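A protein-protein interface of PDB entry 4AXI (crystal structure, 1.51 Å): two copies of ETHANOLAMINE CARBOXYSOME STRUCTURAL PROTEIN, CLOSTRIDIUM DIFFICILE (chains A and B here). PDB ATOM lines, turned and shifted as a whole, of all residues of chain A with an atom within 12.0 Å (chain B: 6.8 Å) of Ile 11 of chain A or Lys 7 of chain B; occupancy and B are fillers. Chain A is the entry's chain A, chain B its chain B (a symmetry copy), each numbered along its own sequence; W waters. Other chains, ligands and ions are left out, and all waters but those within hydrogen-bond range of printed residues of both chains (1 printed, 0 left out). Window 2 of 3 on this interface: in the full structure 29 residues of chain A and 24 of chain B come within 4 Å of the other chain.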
ATOM      1  N   GLU A   4      21.307  11.093   5.420  1.00  0.00           N
ATOM      2  CA  GLU A   4      21.535  10.965   3.995  1.00  0.00           C
ATOM      3  C   GLU A   4      20.719   9.818   3.443  1.00  0.00           C
ATOM      4  O   GLU A   4      20.090   9.946   2.402  1.00  0.00           O
ATOM      5  CB  GLU A   4      23.027  10.708   3.725  1.00  0.00           C
ATOM      6  CG  GLU A   4      23.428  10.688   2.237  1.00  0.00           C
ATOM      7  CD  GLU A   4      23.308   9.310   1.566  1.00  0.00           C
ATOM      8  OE1 GLU A   4      23.033   8.300   2.258  1.00  0.00           O
ATOM      9  OE2 GLU A   4      23.519   9.228   0.335  1.00  0.00           O
ATOM     10  N   LYS A   7      16.596  10.255   2.518  1.00  0.00           N
ATOM     11  CA  LYS A   7      16.100  11.312   1.656  1.00  0.00           C
ATOM     12  C   LYS A   7      15.718  10.762   0.273  1.00  0.00           C
ATOM     13  O   LYS A   7      16.523  10.077  -0.386  1.00  0.00           O
ATOM     14  CB  LYS A   7      17.155  12.416   1.518  1.00  0.00           C
ATOM     15  CG  LYS A   7      17.451  13.258   2.793  1.00  0.00           C
ATOM     16  CD  LYS A   7      18.816  14.004   2.685  1.00  0.00           C
ATOM     17  CE  LYS A   7      19.165  14.738   3.978  1.00  0.00           C
ATOM     18  NZ  LYS A   7      20.492  15.447   3.930  1.00  0.00           N
ATOM     19  N   GLN A   8      14.501  11.070  -0.168  1.00  0.00           N
ATOM     20  CA  GLN A   8      14.102  10.790  -1.538  1.00  0.00           C
ATOM     21  C   GLN A   8      14.968  11.606  -2.505  1.00  0.00           C
ATOM     22  O   GLN A   8      15.401  12.687  -2.178  1.00  0.00           O
ATOM     23  CB  GLN A   8      12.661  11.184  -1.778  1.00  0.00           C
ATOM     24  CG  GLN A   8      12.112  10.637  -3.088  1.00  0.00           C
ATOM     25  CD  GLN A   8      10.755  11.219  -3.481  1.00  0.00           C
ATOM     26  OE1 GLN A   8      10.176  12.052  -2.772  1.00  0.00           O
ATOM     27  NE2 GLN A   8      10.246  10.768  -4.629  1.00  0.00           N
ATOM     28  N   ARG A   9      15.200  11.042  -3.674  1.00  0.00           N
ATOM     29  CA  ARG A   9      16.049  11.647  -4.712  1.00  0.00           C
ATOM     30  C   ARG A   9      15.226  11.674  -6.016  1.00  0.00           C
ATOM     31  O   ARG A   9      14.691  10.625  -6.430  1.00  0.00           O
ATOM     32  CB  ARG A   9      17.297  10.764  -4.831  1.00  0.00           C
ATOM     33  CG  ARG A   9      18.488  11.276  -5.412  1.00  0.00           C
ATOM     34  CD  ARG A   9      19.591  10.208  -5.294  1.00  0.00           C
ATOM     35  NE  ARG A   9      20.567  10.499  -4.248  1.00  0.00           N
ATOM     36  CZ  ARG A   9      21.590  11.347  -4.375  1.00  0.00           C
ATOM     37  NH1 ARG A   9      21.805  11.976  -5.523  1.00  0.00           N
ATOM     38  NH2 ARG A   9      22.442  11.508  -3.363  1.00  0.00           N
ATOM     39  N   VAL A  10      15.131  12.847  -6.647  1.00  0.00           N
ATOM     40  CA  VAL A  10      14.387  13.049  -7.884  1.00  0.00           C
ATOM     41  C   VAL A  10      15.306  13.749  -8.847  1.00  0.00           C
ATOM     42  O   VAL A  10      16.209  14.458  -8.368  1.00  0.00           O
ATOM     43  CB  VAL A  10      13.112  13.879  -7.653  1.00  0.00           C
ATOM     44  CG1 VAL A  10      12.395  14.239  -8.980  1.00  0.00           C
ATOM     45  CG2 VAL A  10      12.170  13.092  -6.764  1.00  0.00           C
ATOM     46  N   ILE A  11      15.171  13.502 -10.145  1.00  0.00           N
ATOM     47  CA  ILE A  11      15.875  14.289 -11.160  1.00  0.00           C
ATOM     48  C   ILE A  11      14.920  15.382 -11.558  1.00  0.00           C
ATOM     49  O   ILE A  11      13.747  15.135 -11.916  1.00  0.00           O
ATOM     50  CB  ILE A  11      16.251  13.448 -12.398  1.00  0.00           C
ATOM     51  CG1 ILE A  11      17.305  12.381 -12.041  1.00  0.00           C
ATOM     52  CG2 ILE A  11      16.763  14.340 -13.497  1.00  0.00           C
ATOM     53  CD1 ILE A  11      17.437  11.285 -13.116  1.00  0.00           C
ATOM     54  N   GLN A  12      15.365  16.641 -11.500  1.00  0.00           N
ATOM     55  CA  GLN A  12      14.530  17.774 -11.897  1.00  0.00           C
ATOM     56  C   GLN A  12      15.159  18.391 -13.132  1.00  0.00           C
ATOM     57  O   GLN A  12      16.293  18.830 -13.074  1.00  0.00           O
ATOM     58  CB  GLN A  12      14.496  18.798 -10.725  1.00  0.00           C
ATOM     59  CG  GLN A  12      14.466  20.312 -11.041  1.00  0.00           C
ATOM     60  CD  GLN A  12      15.785  21.055 -10.740  1.00  0.00           C
ATOM     61  OE1 GLN A  12      16.528  21.358 -11.658  1.00  0.00           O
ATOM     62  NE2 GLN A  12      16.058  21.365  -9.459  1.00  0.00           N
ATOM     63  N   GLU A  13      14.408  18.429 -14.229  1.00  0.00           N
ATOM     64  CA  GLU A  13      14.840  19.058 -15.477  1.00  0.00           C
ATOM     65  C   GLU A  13      14.387  20.497 -15.402  1.00  0.00           C
ATOM     66  O   GLU A  13      13.180  20.763 -15.416  1.00  0.00           O
ATOM     67  CB  GLU A  13      14.159  18.371 -16.679  1.00  0.00           C
ATOM     68  CG  GLU A  13      14.427  16.879 -16.708  1.00  0.00           C
ATOM     69  CD  GLU A  13      14.054  16.220 -18.028  1.00  0.00           C
ATOM     70  OE1 GLU A  13      13.744  16.922 -18.980  1.00  0.00           O
ATOM     71  OE2 GLU A  13      14.089  14.981 -18.075  1.00  0.00           O
ATOM     72  N   TYR A  14      15.311  21.443 -15.319  1.00  0.00           N
ATOM     73  CA  TYR A  14      14.891  22.823 -15.142  1.00  0.00           C
ATOM     74  C   TYR A  14      14.632  23.563 -16.463  1.00  0.00           C
ATOM     75  O   TYR A  14      15.377  23.418 -17.449  1.00  0.00           O
ATOM     76  CB  TYR A  14      15.916  23.585 -14.311  1.00  0.00           C
ATOM     77  CG  TYR A  14      17.359  23.577 -14.837  1.00  0.00           C
ATOM     78  CD1 TYR A  14      17.789  24.496 -15.809  1.00  0.00           C
ATOM     79  CD2 TYR A  14      18.293  22.699 -14.303  1.00  0.00           C
ATOM     80  CE1 TYR A  14      19.092  24.535 -16.213  1.00  0.00           C
ATOM     81  CE2 TYR A  14      19.653  22.752 -14.690  1.00  0.00           C
ATOM     82  CZ  TYR A  14      20.021  23.663 -15.687  1.00  0.00           C
ATOM     83  OH  TYR A  14      21.325  23.785 -16.110  1.00  0.00           O
ATOM     84  N   VAL A  15      13.551  24.335 -16.473  1.00  0.00           N
ATOM     85  CA  VAL A  15      13.210  25.236 -17.571  1.00  0.00           C
ATOM     86  C   VAL A  15      12.651  26.474 -16.910  1.00  0.00           C
ATOM     87  O   VAL A  15      12.089  26.430 -15.842  1.00  0.00           O
ATOM     88  CB  VAL A  15      12.201  24.611 -18.584  1.00  0.00           C
ATOM     89  CG1 VAL A  15      12.711  23.309 -19.173  1.00  0.00           C
ATOM     90  CG2 VAL A  15      10.860  24.392 -17.905  1.00  0.00           C
ATOM     91  N   THR B   3      20.518   4.100  -8.461  1.00  0.00           N
ATOM     92  CA  THR B   3      20.733   3.979  -9.920  1.00  0.00           C
ATOM     93  C   THR B   3      19.984   5.010 -10.748  1.00  0.00           C
ATOM     94  O   THR B   3      18.869   5.435 -10.408  1.00  0.00           O
ATOM     95  CB  THR B   3      20.255   2.605 -10.501  1.00  0.00           C
ATOM     96  OG1 THR B   3      18.862   2.443 -10.271  1.00  0.00           O
ATOM     97  CG2 THR B   3      20.966   1.450  -9.894  1.00  0.00           C
ATOM     98  N   GLU B   4      20.612   5.407 -11.851  1.00  0.00           N
ATOM     99  CA  GLU B   4      20.010   6.330 -12.800  1.00  0.00           C
ATOM    100  C   GLU B   4      18.599   5.909 -13.148  1.00  0.00           C
ATOM    101  O   GLU B   4      17.695   6.728 -13.196  1.00  0.00           O
ATOM    102  CB  GLU B   4      20.840   6.400 -14.092  1.00  0.00           C
ATOM    103  CG  GLU B   4      20.269   7.402 -15.126  1.00  0.00           C
ATOM    104  CD  GLU B   4      19.696   6.753 -16.404  1.00  0.00           C
ATOM    105  OE1 GLU B   4      19.825   5.513 -16.549  1.00  0.00           O
ATOM    106  OE2 GLU B   4      19.120   7.490 -17.261  1.00  0.00           O
ATOM    107  N   GLU B   5      18.424   4.606 -13.357  1.00  0.00           N
ATOM    108  CA  GLU B   5      17.179   4.062 -13.884  1.00  0.00           C
ATOM    109  C   GLU B   5      16.010   4.138 -12.899  1.00  0.00           C
ATOM    110  O   GLU B   5      14.860   4.108 -13.300  1.00  0.00           O
ATOM    111  CB  GLU B   5      17.395   2.606 -14.313  1.00  0.00           C
ATOM    112  CG  GLU B   5      18.332   2.420 -15.500  1.00  0.00           C
ATOM    113  CD  GLU B   5      19.818   2.245 -15.145  1.00  0.00           C
ATOM    114  OE1 GLU B   5      20.262   2.581 -14.026  1.00  0.00           O
ATOM    115  OE2 GLU B   5      20.560   1.778 -16.037  1.00  0.00           O
ATOM    116  N   SER B   6      16.316   4.257 -11.615  1.00  0.00           N
ATOM    117  CA  SER B   6      15.308   4.213 -10.559  1.00  0.00           C
ATOM    118  C   SER B   6      14.780   5.585 -10.134  1.00  0.00           C
ATOM    119  O   SER B   6      13.929   5.666  -9.257  1.00  0.00           O
ATOM    120  CB  SER B   6      15.907   3.549  -9.307  1.00  0.00           C
ATOM    121  OG  SER B   6      16.928   4.379  -8.713  1.00  0.00           O
ATOM    122  N   LYS B   7      15.341   6.651 -10.694  1.00  0.00           N
ATOM    123  CA  LYS B   7      14.976   8.008 -10.274  1.00  0.00           C
ATOM    124  C   LYS B   7      13.796   8.574 -11.093  1.00  0.00           C
ATOM    125  O   LYS B   7      13.795   8.515 -12.321  1.00  0.00           O
ATOM    126  CB  LYS B   7      16.202   8.926 -10.389  1.00  0.00           C
ATOM    127  CG  LYS B   7      17.365   8.622  -9.413  1.00  0.00           C
ATOM    128  CD  LYS B   7      18.731   9.186  -9.937  1.00  0.00           C
ATOM    129  CE  LYS B   7      19.909   8.702  -9.111  1.00  0.00           C
ATOM    130  NZ  LYS B   7      21.207   9.297  -9.554  1.00  0.00           N
ATOM    131  N   GLN B   8      12.795   9.109 -10.402  1.00  0.00           N
ATOM    132  CA  GLN B   8      11.719   9.838 -11.054  1.00  0.00           C
ATOM    133  C   GLN B   8      12.325  11.117 -11.637  1.00  0.00           C
ATOM    134  O   GLN B   8      13.278  11.638 -11.056  1.00  0.00           O
ATOM    135  CB  GLN B   8      10.675  10.246 -10.032  1.00  0.00           C
ATOM    136  CG  GLN B   8       9.322  10.678 -10.647  1.00  0.00           C
ATOM    137  CD  GLN B   8       8.419  11.464  -9.667  1.00  0.00           C
ATOM    138  OE1 GLN B   8       8.641  11.461  -8.451  1.00  0.00           O
ATOM    139  NE2 GLN B   8       7.396  12.119 -10.204  1.00  0.00           N
ATOM    140  N   ARG B   9      11.780  11.526 -12.778  1.00  0.00           N
ATOM    141  CA  ARG B   9      12.151  12.756 -13.487  1.00  0.00           C
ATOM    142  C   ARG B   9      10.942  13.605 -13.581  1.00  0.00           C
ATOM    143  O   ARG B   9       9.862  13.140 -14.005  1.00  0.00           O
ATOM    144  CB  ARG B   9      12.537  12.537 -14.949  1.00  0.00           C
ATOM    145  CG  ARG B   9      13.815  11.988 -15.194  1.00  0.00           C
ATOM    146  CD  ARG B   9      14.070  11.837 -16.679  1.00  0.00           C
ATOM    147  NE  ARG B   9      15.447  11.467 -16.706  1.00  0.00           N
ATOM    148  CZ  ARG B   9      16.477  12.271 -16.959  1.00  0.00           C
ATOM    149  NH1 ARG B   9      16.343  13.547 -17.362  1.00  0.00           N
ATOM    150  NH2 ARG B   9      17.652  11.701 -16.875  1.00  0.00           N
ATOM    151  N   VAL B  10      11.105  14.869 -13.235  1.00  0.00           N
ATOM    152  CA  VAL B  10      10.049  15.843 -13.411  1.00  0.00           C
ATOM    153  C   VAL B  10      10.588  17.076 -14.052  1.00  0.00           C
ATOM    154  O   VAL B  10      11.767  17.386 -13.880  1.00  0.00           O
ATOM    155  CB  VAL B  10       9.433  16.263 -12.089  1.00  0.00           C
ATOM    156  CG1 VAL B  10       8.780  15.095 -11.412  1.00  0.00           C
ATOM    157  CG2 VAL B  10      10.480  16.847 -11.198  1.00  0.00           C
ATOM    158  N   ILE B  11       9.785  17.778 -14.806  1.00  0.00           N
ATOM    159  CA  ILE B  11      10.214  19.098 -15.331  1.00  0.00           C
ATOM    160  C   ILE B  11       9.790  20.128 -14.351  1.00  0.00           C
ATOM    161  O   ILE B  11       8.623  20.176 -13.951  1.00  0.00           O
ATOM    162  CB  ILE B  11       9.573  19.359 -16.728  1.00  0.00           C
ATOM    163  CG1 ILE B  11      10.049  18.327 -17.770  1.00  0.00           C
ATOM    164  CG2 ILE B  11       9.820  20.803 -17.192  1.00  0.00           C
ATOM    165  CD1 ILE B  11       9.246  18.344 -19.003  1.00  0.00           C
HETATM  166  O   HOH W   1      12.856   9.156  -7.184  1.00  0.00           O
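Val 10 of chain A touches Gln 8 of chain B, but with the chains exchanged Gln 8 of chain A does not touch Val 10 of chain B (8.2 Å). Val 10 of chain A touches its own counterpart, Val 10 of chain B. Ile 11 of chain A touches Lys 7 of chain B, but with the chains exchanged Lys 7 of chain A does not touch Ile 11 of chain B (17.7 Å). Ile 11 of chain A touches Arg 9 of chain B, but with the chains exchanged Arg 9 of chain A does not touch Ile 11 of chain B (12.0 Å).
The backbone NH of Val 10 of chain B is in hydrogen-bond range of the backbone carbonyl oxygen of Ile 11 of chain A (3.0 Å). The backbone NH (N) of Ile 11 of chain A sits at hydrogen-bond distance from the backbone carbonyl oxygen (O) of Gln 8 of chain B. OE2 of Glu 13 of chain A lies within salt-bridge range of NH1 of Arg 9 of chain B (2.8 Å). O of Val 10 of chain B lies within hydrogen-bond range of N of Glu 13 of chain A, at 2.9 Å.
Water W1 lies within hydrogen-bond range of O of Arg 9 of chain A (2.5 Å) and N of Gln 8 of chain B (3.2 Å).
Of the 9 printed residues of chain B, 5 touch a printed residue of chain A. Hydrophobic or aromatic side chains of chain A within 4 Å of the printed part of chain B: Val 10, Ile 11 and Val 15. Among the printed residues, 11 pairs touch across the chains.
Of the printed residues of chain B, Gln 12 of chain A touches Val 10 (3.4 Å). Of the printed residues of chain B, Glu 13 of chain A touches Arg 9 (2.8 Å), Val 10 (2.9 Å) and Ile 11 (3.4 Å). Printed residues of chain B within 4 Å of Val 15 of chain A: Ile 11 (3.8 Å). No residue of chain A comes within 4 Å of Glu 4 of chain B. No residue of chain A comes within 4 Å of Ser 6 of chain B. Lys 7 of chain B touches just one residue of chain A: Ile 11 (3.8 Å). Printed residues of chain A within 4 Å of Val 10 of chain B: Val 10, Ile 11, Gln 12 and Glu 13. Printed residues of chain A within 4 Å of Ile 11 of chain B: Glu 13 and Val 15. The nearest residue of chain B that does not touch Ile 11 of chain A is Glu 4 of chain B (4.6 Å). The nearest residue of chain A that does not touch Lys 7 of chain B is Arg 9 of chain A (4.1 Å).
Among the printed residues, pairs that only touch across the chains: Val 10 of chain A with Gln 8 of chain B (3.4 Å), Val 10 of chain A with Val 10 of chain B (3.9 Å), Ile 11 of chain A with Lys 7 of chain B (3.8 Å), Ile 11 of chain A with Arg 9 of chain B (3.3 Å), Gln 12 of chain A with Val 10 of chain B (3.4 Å), Glu 13 of chain A with Ile 11 of chain B (3.4 Å) and Val 15 of chain A with Ile 11 of chain B (3.8 Å).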
